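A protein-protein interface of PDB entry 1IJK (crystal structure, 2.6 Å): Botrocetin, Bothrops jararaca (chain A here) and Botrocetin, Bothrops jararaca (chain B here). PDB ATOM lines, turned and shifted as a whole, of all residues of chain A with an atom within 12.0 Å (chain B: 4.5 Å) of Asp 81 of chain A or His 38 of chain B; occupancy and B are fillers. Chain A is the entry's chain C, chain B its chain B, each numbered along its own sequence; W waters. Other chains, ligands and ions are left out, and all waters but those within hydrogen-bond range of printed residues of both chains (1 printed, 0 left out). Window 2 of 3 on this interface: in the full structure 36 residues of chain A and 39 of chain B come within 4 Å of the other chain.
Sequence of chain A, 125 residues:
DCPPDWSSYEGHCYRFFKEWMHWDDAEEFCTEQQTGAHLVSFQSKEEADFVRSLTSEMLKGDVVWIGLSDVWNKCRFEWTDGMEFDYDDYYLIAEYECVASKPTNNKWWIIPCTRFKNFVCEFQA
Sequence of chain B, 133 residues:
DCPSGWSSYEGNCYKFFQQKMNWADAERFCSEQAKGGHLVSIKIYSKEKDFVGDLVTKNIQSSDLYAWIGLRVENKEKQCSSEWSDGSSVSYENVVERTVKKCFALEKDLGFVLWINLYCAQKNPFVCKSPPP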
ATOM      1  N   PHE A  77     -20.190 -29.506 -17.434  1.00  0.00           N
ATOM      2  CA  PHE A  77     -20.721 -28.962 -18.686  1.00  0.00           C
ATOM      3  C   PHE A  77     -21.538 -29.989 -19.442  1.00  0.00           C
ATOM      4  O   PHE A  77     -21.309 -31.187 -19.314  1.00  0.00           O
ATOM      5  CB  PHE A  77     -19.580 -28.476 -19.587  1.00  0.00           C
ATOM      6  CG  PHE A  77     -18.601 -27.586 -18.892  1.00  0.00           C
ATOM      7  CD1 PHE A  77     -17.315 -28.028 -18.624  1.00  0.00           C
ATOM      8  CD2 PHE A  77     -18.973 -26.308 -18.475  1.00  0.00           C
ATOM      9  CE1 PHE A  77     -16.417 -27.217 -17.956  1.00  0.00           C
ATOM     10  CE2 PHE A  77     -18.071 -25.487 -17.799  1.00  0.00           C
ATOM     11  CZ  PHE A  77     -16.796 -25.945 -17.543  1.00  0.00           C
ATOM     12  N   GLU A  78     -22.486 -29.505 -20.237  1.00  0.00           N
ATOM     13  CA  GLU A  78     -23.340 -30.368 -21.046  1.00  0.00           C
ATOM     14  C   GLU A  78     -23.788 -29.616 -22.296  1.00  0.00           C
ATOM     15  O   GLU A  78     -24.126 -28.438 -22.226  1.00  0.00           O
ATOM     16  CB  GLU A  78     -24.581 -30.780 -20.261  1.00  0.00           C
ATOM     17  CG  GLU A  78     -25.500 -29.621 -19.953  1.00  0.00           C
ATOM     18  CD  GLU A  78     -26.699 -30.019 -19.121  1.00  0.00           C
ATOM     19  OE1 GLU A  78     -27.516 -29.126 -18.803  1.00  0.00           O
ATOM     20  OE2 GLU A  78     -26.827 -31.217 -18.786  1.00  0.00           O
ATOM     21  N   TRP A  79     -23.781 -30.284 -23.443  1.00  0.00           N
ATOM     22  CA  TRP A  79     -24.247 -29.627 -24.651  1.00  0.00           C
ATOM     23  C   TRP A  79     -25.740 -29.832 -24.728  1.00  0.00           C
ATOM     24  O   TRP A  79     -26.257 -30.867 -24.322  1.00  0.00           O
ATOM     25  CB  TRP A  79     -23.581 -30.191 -25.889  1.00  0.00           C
ATOM     26  CG  TRP A  79     -22.118 -29.956 -25.911  1.00  0.00           C
ATOM     27  CD1 TRP A  79     -21.163 -30.741 -25.354  1.00  0.00           C
ATOM     28  CD2 TRP A  79     -21.435 -28.874 -26.547  1.00  0.00           C
ATOM     29  NE1 TRP A  79     -19.919 -30.226 -25.608  1.00  0.00           N
ATOM     30  CE2 TRP A  79     -20.053 -29.078 -26.339  1.00  0.00           C
ATOM     31  CE3 TRP A  79     -21.856 -27.753 -27.274  1.00  0.00           C
ATOM     32  CZ2 TRP A  79     -19.080 -28.203 -26.834  1.00  0.00           C
ATOM     33  CZ3 TRP A  79     -20.894 -26.882 -27.768  1.00  0.00           C
ATOM     34  CH2 TRP A  79     -19.515 -27.114 -27.545  1.00  0.00           C
ATOM     35  N   THR A  80     -26.430 -28.831 -25.246  1.00  0.00           N
ATOM     36  CA  THR A  80     -27.874 -28.866 -25.350  1.00  0.00           C
ATOM     37  C   THR A  80     -28.406 -30.058 -26.184  1.00  0.00           C
ATOM     38  O   THR A  80     -29.589 -30.407 -26.096  1.00  0.00           O
ATOM     39  CB  THR A  80     -28.351 -27.507 -25.903  1.00  0.00           C
ATOM     40  OG1 THR A  80     -29.710 -27.292 -25.545  1.00  0.00           O
ATOM     41  CG2 THR A  80     -28.211 -27.459 -27.401  1.00  0.00           C
ATOM     42  N   ASP A  81     -27.538 -30.683 -26.986  1.00  0.00           N
ATOM     43  CA  ASP A  81     -27.944 -31.836 -27.789  1.00  0.00           C
ATOM     44  C   ASP A  81     -27.355 -33.119 -27.211  1.00  0.00           C
ATOM     45  O   ASP A  81     -27.276 -34.148 -27.891  1.00  0.00           O
ATOM     46  CB  ASP A  81     -27.507 -31.696 -29.255  1.00  0.00           C
ATOM     47  CG  ASP A  81     -26.008 -31.797 -29.441  1.00  0.00           C
ATOM     48  OD1 ASP A  81     -25.323 -32.393 -28.586  1.00  0.00           O
ATOM     49  OD2 ASP A  81     -25.504 -31.295 -30.467  1.00  0.00           O
ATOM     50  N   GLY A  82     -26.923 -33.035 -25.958  1.00  0.00           N
ATOM     51  CA  GLY A  82     -26.359 -34.182 -25.281  1.00  0.00           C
ATOM     52  C   GLY A  82     -25.070 -34.705 -25.871  1.00  0.00           C
ATOM     53  O   GLY A  82     -24.700 -35.850 -25.618  1.00  0.00           O
ATOM     54  N   MET A  83     -24.369 -33.891 -26.652  1.00  0.00           N
ATOM     55  CA  MET A  83     -23.125 -34.375 -27.225  1.00  0.00           C
ATOM     56  C   MET A  83     -22.214 -34.887 -26.116  1.00  0.00           C
ATOM     57  O   MET A  83     -22.217 -34.368 -25.001  1.00  0.00           O
ATOM     58  CB  MET A  83     -22.405 -33.291 -28.019  1.00  0.00           C
ATOM     59  CG  MET A  83     -21.144 -33.835 -28.664  1.00  0.00           C
ATOM     60  SD  MET A  83     -20.224 -32.669 -29.650  1.00  0.00           S
ATOM     61  CE  MET A  83     -19.777 -31.484 -28.391  1.00  0.00           C
ATOM     62  N   GLU A  84     -21.438 -35.916 -26.438  1.00  0.00           N
ATOM     63  CA  GLU A  84     -20.524 -36.541 -25.494  1.00  0.00           C
ATOM     64  C   GLU A  84     -19.126 -35.957 -25.658  1.00  0.00           C
ATOM     65  O   GLU A  84     -18.611 -35.863 -26.768  1.00  0.00           O
ATOM     66  CB  GLU A  84     -20.493 -38.054 -25.748  1.00  0.00           C
ATOM     67  CG  GLU A  84     -20.421 -38.925 -24.493  1.00  0.00           C
ATOM     68  CD  GLU A  84     -21.599 -38.704 -23.555  1.00  0.00           C
ATOM     69  OE1 GLU A  84     -22.755 -38.768 -24.029  1.00  0.00           O
ATOM     70  OE2 GLU A  84     -21.369 -38.470 -22.343  1.00  0.00           O
ATOM     71  N   PHE A  85     -18.515 -35.556 -24.549  1.00  0.00           N
ATOM     72  CA  PHE A  85     -17.172 -34.987 -24.596  1.00  0.00           C
ATOM     73  C   PHE A  85     -16.320 -35.536 -23.460  1.00  0.00           C
ATOM     74  O   PHE A  85     -16.832 -36.116 -22.502  1.00  0.00           O
ATOM     75  CB  PHE A  85     -17.237 -33.461 -24.498  1.00  0.00           C
ATOM     76  CG  PHE A  85     -17.786 -32.962 -23.194  1.00  0.00           C
ATOM     77  CD1 PHE A  85     -16.936 -32.627 -22.149  1.00  0.00           C
ATOM     78  CD2 PHE A  85     -19.152 -32.830 -23.009  1.00  0.00           C
ATOM     79  CE1 PHE A  85     -17.438 -32.161 -20.941  1.00  0.00           C
ATOM     80  CE2 PHE A  85     -19.668 -32.370 -21.802  1.00  0.00           C
ATOM     81  CZ  PHE A  85     -18.811 -32.033 -20.767  1.00  0.00           C
ATOM     82  N   ASP A  86     -15.016 -35.341 -23.579  1.00  0.00           N
ATOM     83  CA  ASP A  86     -14.072 -35.798 -22.578  1.00  0.00           C
ATOM     84  C   ASP A  86     -13.529 -34.588 -21.820  1.00  0.00           C
ATOM     85  O   ASP A  86     -12.748 -33.812 -22.367  1.00  0.00           O
ATOM     86  CB  ASP A  86     -12.953 -36.583 -23.278  1.00  0.00           C
ATOM     87  CG  ASP A  86     -11.691 -36.674 -22.457  1.00  0.00           C
ATOM     88  OD1 ASP A  86     -11.779 -36.802 -21.215  1.00  0.00           O
ATOM     89  OD2 ASP A  86     -10.597 -36.630 -23.062  1.00  0.00           O
ATOM     90  N   TYR A  90     -11.439 -30.240 -22.140  1.00  0.00           N
ATOM     91  CA  TYR A  90     -11.911 -28.911 -21.765  1.00  0.00           C
ATOM     92  C   TYR A  90     -10.994 -28.246 -20.753  1.00  0.00           C
ATOM     93  O   TYR A  90     -11.294 -28.196 -19.563  1.00  0.00           O
ATOM     94  CB  TYR A  90     -13.336 -28.992 -21.212  1.00  0.00           C
ATOM     95  CG  TYR A  90     -14.366 -29.337 -22.263  1.00  0.00           C
ATOM     96  CD1 TYR A  90     -15.727 -29.289 -21.974  1.00  0.00           C
ATOM     97  CD2 TYR A  90     -13.977 -29.709 -23.557  1.00  0.00           C
ATOM     98  CE1 TYR A  90     -16.685 -29.599 -22.943  1.00  0.00           C
ATOM     99  CE2 TYR A  90     -14.919 -30.026 -24.525  1.00  0.00           C
ATOM    100  CZ  TYR A  90     -16.272 -29.969 -24.209  1.00  0.00           C
ATOM    101  OH  TYR A  90     -17.204 -30.283 -25.161  1.00  0.00           O
ATOM    102  N   GLU B  27     -31.645 -21.356 -27.884  1.00  0.00           N
ATOM    103  CA  GLU B  27     -31.769 -22.807 -27.828  1.00  0.00           C
ATOM    104  C   GLU B  27     -33.167 -23.260 -28.265  1.00  0.00           C
ATOM    105  O   GLU B  27     -33.312 -24.206 -29.047  1.00  0.00           O
ATOM    106  CB  GLU B  27     -31.471 -23.285 -26.407  1.00  0.00           C
ATOM    107  CG  GLU B  27     -31.894 -24.698 -26.077  1.00  0.00           C
ATOM    108  CD  GLU B  27     -31.390 -25.715 -27.057  1.00  0.00           C
ATOM    109  OE1 GLU B  27     -30.327 -25.479 -27.666  1.00  0.00           O
ATOM    110  OE2 GLU B  27     -32.054 -26.767 -27.210  1.00  0.00           O
ATOM    111  N   CYS B  30     -33.637 -22.748 -32.070  1.00  0.00           N
ATOM    112  CA  CYS B  30     -33.000 -23.772 -32.888  1.00  0.00           C
ATOM    113  C   CYS B  30     -33.774 -25.087 -32.910  1.00  0.00           C
ATOM    114  O   CYS B  30     -33.764 -25.803 -33.904  1.00  0.00           O
ATOM    115  CB  CYS B  30     -31.584 -24.041 -32.392  1.00  0.00           C
ATOM    116  SG  CYS B  30     -30.388 -22.706 -32.680  1.00  0.00           S
ATOM    117  N   GLY B  36     -34.743 -32.265 -33.859  1.00  0.00           N
ATOM    118  CA  GLY B  36     -33.400 -32.539 -33.386  1.00  0.00           C
ATOM    119  C   GLY B  36     -32.475 -31.347 -33.554  1.00  0.00           C
ATOM    120  O   GLY B  36     -31.256 -31.512 -33.617  1.00  0.00           O
ATOM    121  N   GLY B  37     -33.061 -30.150 -33.624  1.00  0.00           N
ATOM    122  CA  GLY B  37     -32.282 -28.934 -33.778  1.00  0.00           C
ATOM    123  C   GLY B  37     -31.913 -28.341 -32.434  1.00  0.00           C
ATOM    124  O   GLY B  37     -32.721 -28.310 -31.516  1.00  0.00           O
ATOM    125  N   HIS B  38     -30.680 -27.854 -32.340  1.00  0.00           N
ATOM    126  CA  HIS B  38     -30.136 -27.274 -31.114  1.00  0.00           C
ATOM    127  C   HIS B  38     -29.077 -26.247 -31.432  1.00  0.00           C
ATOM    128  O   HIS B  38     -28.582 -26.176 -32.554  1.00  0.00           O
ATOM    129  CB  HIS B  38     -29.426 -28.352 -30.283  1.00  0.00           C
ATOM    130  CG  HIS B  38     -30.345 -29.303 -29.596  1.00  0.00           C
ATOM    131  ND1 HIS B  38     -31.182 -28.916 -28.571  1.00  0.00           N
ATOM    132  CD2 HIS B  38     -30.550 -30.628 -29.774  1.00  0.00           C
ATOM    133  CE1 HIS B  38     -31.864 -29.964 -28.147  1.00  0.00           C
ATOM    134  NE2 HIS B  38     -31.499 -31.016 -28.859  1.00  0.00           N
ATOM    135  N   LEU B  39     -28.709 -25.467 -30.421  1.00  0.00           N
ATOM    136  CA  LEU B  39     -27.628 -24.525 -30.590  1.00  0.00           C
ATOM    137  C   LEU B  39     -26.497 -25.461 -30.988  1.00  0.00           C
ATOM    138  O   LEU B  39     -26.358 -26.542 -30.446  1.00  0.00           O
ATOM    139  CB  LEU B  39     -27.298 -23.815 -29.270  1.00  0.00           C
ATOM    140  CG  LEU B  39     -28.037 -22.495 -29.049  1.00  0.00           C
ATOM    141  CD1 LEU B  39     -27.721 -21.927 -27.683  1.00  0.00           C
ATOM    142  CD2 LEU B  39     -27.642 -21.515 -30.147  1.00  0.00           C
ATOM    143  N   VAL B  40     -25.708 -25.055 -31.957  1.00  0.00           N
ATOM    144  CA  VAL B  40     -24.618 -25.872 -32.442  1.00  0.00           C
ATOM    145  C   VAL B  40     -23.752 -26.488 -31.318  1.00  0.00           C
ATOM    146  O   VAL B  40     -23.537 -25.876 -30.278  1.00  0.00           O
ATOM    147  CB  VAL B  40     -23.754 -25.016 -33.382  1.00  0.00           C
ATOM    148  CG1 VAL B  40     -23.122 -23.879 -32.581  1.00  0.00           C
ATOM    149  CG2 VAL B  40     -22.716 -25.868 -34.081  1.00  0.00           C
ATOM    150  N   SER B  41     -23.296 -27.718 -31.535  1.00  0.00           N
ATOM    151  CA  SER B  41     -22.423 -28.422 -30.605  1.00  0.00           C
ATOM    152  C   SER B  41     -21.169 -28.597 -31.440  1.00  0.00           C
ATOM    153  O   SER B  41     -21.261 -28.824 -32.643  1.00  0.00           O
ATOM    154  CB  SER B  41     -23.000 -29.786 -30.219  1.00  0.00           C
ATOM    155  OG  SER B  41     -23.216 -30.603 -31.356  1.00  0.00           O
ATOM    156  N   VAL B 127     -25.657 -19.912 -33.713  1.00  0.00           N
ATOM    157  CA  VAL B 127     -25.551 -20.919 -34.747  1.00  0.00           C
ATOM    158  C   VAL B 127     -26.433 -22.084 -34.328  1.00  0.00           C
ATOM    159  O   VAL B 127     -26.376 -22.539 -33.184  1.00  0.00           O
ATOM    160  CB  VAL B 127     -24.105 -21.406 -34.932  1.00  0.00           C
ATOM    161  CG1 VAL B 127     -24.054 -22.514 -35.991  1.00  0.00           C
ATOM    162  CG2 VAL B 127     -23.227 -20.253 -35.358  1.00  0.00           C
ATOM    163  N   CYS B 128     -27.275 -22.539 -35.253  1.00  0.00           N
ATOM    164  CA  CYS B 128     -28.173 -23.652 -34.996  1.00  0.00           C
ATOM    165  C   CYS B 128     -27.632 -24.887 -35.675  1.00  0.00           C
ATOM    166  O   CYS B 128     -26.913 -24.800 -36.664  1.00  0.00           O
ATOM    167  CB  CYS B 128     -29.573 -23.382 -35.551  1.00  0.00           C
ATOM    168  SG  CYS B 128     -30.628 -22.212 -34.638  1.00  0.00           S
ATOM    169  N   LYS B 129     -27.993 -26.040 -35.135  1.00  0.00           N
ATOM    170  CA  LYS B 129     -27.563 -27.306 -35.696  1.00  0.00           C
ATOM    171  C   LYS B 129     -28.667 -28.334 -35.542  1.00  0.00           C
ATOM    172  O   LYS B 129     -29.161 -28.585 -34.439  1.00  0.00           O
ATOM    173  CB  LYS B 129     -26.297 -27.800 -34.996  1.00  0.00           C
ATOM    174  CG  LYS B 129     -25.839 -29.179 -35.424  1.00  0.00           C
ATOM    175  CD  LYS B 129     -24.441 -29.457 -34.895  1.00  0.00           C
ATOM    176  CE  LYS B 129     -23.976 -30.869 -35.232  1.00  0.00           C
ATOM    177  NZ  LYS B 129     -22.535 -31.086 -34.910  1.00  0.00           N
HETATM  178  O   HOH W   1     -25.948 -28.966 -31.936  1.00  0.00           O
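The side-chain carboxylate (OE1) of Glu 27 of chain B sits close to the side-chain hydroxyl (OG1) of Thr 80 of chain A, 2.9 Å away.
The backbone carbonyl oxygen (O) of Thr 80 of chain A sits close to a ring nitrogen (ND1) of His 38 of chain B, at 3.3 Å.
OD2 of Asp 81 of chain A is in hydrogen-bond range of OG of Ser 41 of chain B, at 2.6 Å.
OE2 of Glu 27 of chain B lies within hydrogen-bond range of ND1 of His 38 of chain B, at 2.7 Å.
The backbone carbonyl oxygen (O) of Val 127 of chain B sits at hydrogen-bond distance from the backbone NH (N) of Val 40 of chain B (2.9 Å).
The backbone carbonyl oxygen (O) of Ser 41 of chain B lies within hydrogen-bond range of the side-chain amino group (NZ) of Lys 129 of chain B (3.4 Å).
The side-chain hydroxyl of Tyr 90 of chain A lies within hydrogen-bond range of the indole nitrogen of Trp 79 of chain A (2.8 Å).
The side-chain carboxylate (OD1) of Asp 81 of chain A sits at hydrogen-bond distance from the backbone NH (N) of Met 83 of chain A (2.6 Å).
The side-chain sulfur (SG) of Cys 30 of chain B forms a disulfide with the side-chain sulfur (SG) of Cys 128 of chain B (2.0 Å).
O of Val 40 of chain B touches CZ3 of Trp 79 of chain A, 3.8 Å away.
CE3 of Trp 79 of chain A touches CA of Ser 41 of chain B, at 3.4 Å.
Thr 80 of chain A touches Leu 39 of chain B (CG2 to N, 3.7 Å).
Asp 81 of chain A touches His 38 of chain B (CB to CD2, 3.3 Å).
Printed residues of chain B within 4 Å of Trp 79 of chain A: Val 40 and Ser 41.
Of the printed residues of chain B, Thr 80 of chain A touches Glu 27 (2.8 Å), His 38 (3.1 Å) and Leu 39 (3.7 Å).
Of the printed residues of chain B, Asp 81 of chain A touches His 38 and Ser 41.
Asp 86 of chain A touches none of the printed residues of chain B.
No residue of chain A comes within 4 Å of Cys 30 of chain B.
No residue of chain A comes within 4 Å of Gly 37 of chain B.
Of chain A, only Thr 80 (3.1 Å) and Asp 81 (3.3 Å) come within 4 Å of His 38 of chain B.
Of chain A, only Thr 80 comes within 4 Å of Leu 39 of chain B.
Val 40 of chain B touches one residue of chain A.
Printed residues of chain A within 4 Å of Ser 41 of chain B: Trp 79 (3.4 Å) and Asp 81 (2.6 Å).
No residue of chain A comes within 4 Å of Cys 128 of chain B.
No residue of chain A comes within 4 Å of Lys 129 of chain B.
The nearest printed residue of chain B that does not touch Asp 81 of chain A is Leu 39 of chain B (4.8 Å).
The nearest residue of chain A that does not touch His 38 of chain B is Gly 82 of chain A (5.8 Å).
Of the 11 printed residues of chain B, 5 touch a printed residue of chain A.
Hydrophobic or aromatic side chains of chain B within 4 Å of the printed part of chain A: His 38.
Of the 11 printed residues of chain A, 3 touch a printed residue of chain B.
Printed residues of chain A that touch a printed residue of chain B: Trp 79, Thr 80 and Asp 81.
Hydrophobic or aromatic side chains of chain A that line the printed part of chain B: Trp 79.
Among the printed residues, no Asp or Glu carboxylate lies within 4 Å of a Lys or Arg side-chain nitrogen of the other chain.
Water W1 lies within hydrogen-bond range of the side-chain carboxylate of Asp 81 of chain A, the backbone carbonyl oxygen of Leu 39 of chain B and the backbone NH of Ser 41 of chain B.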
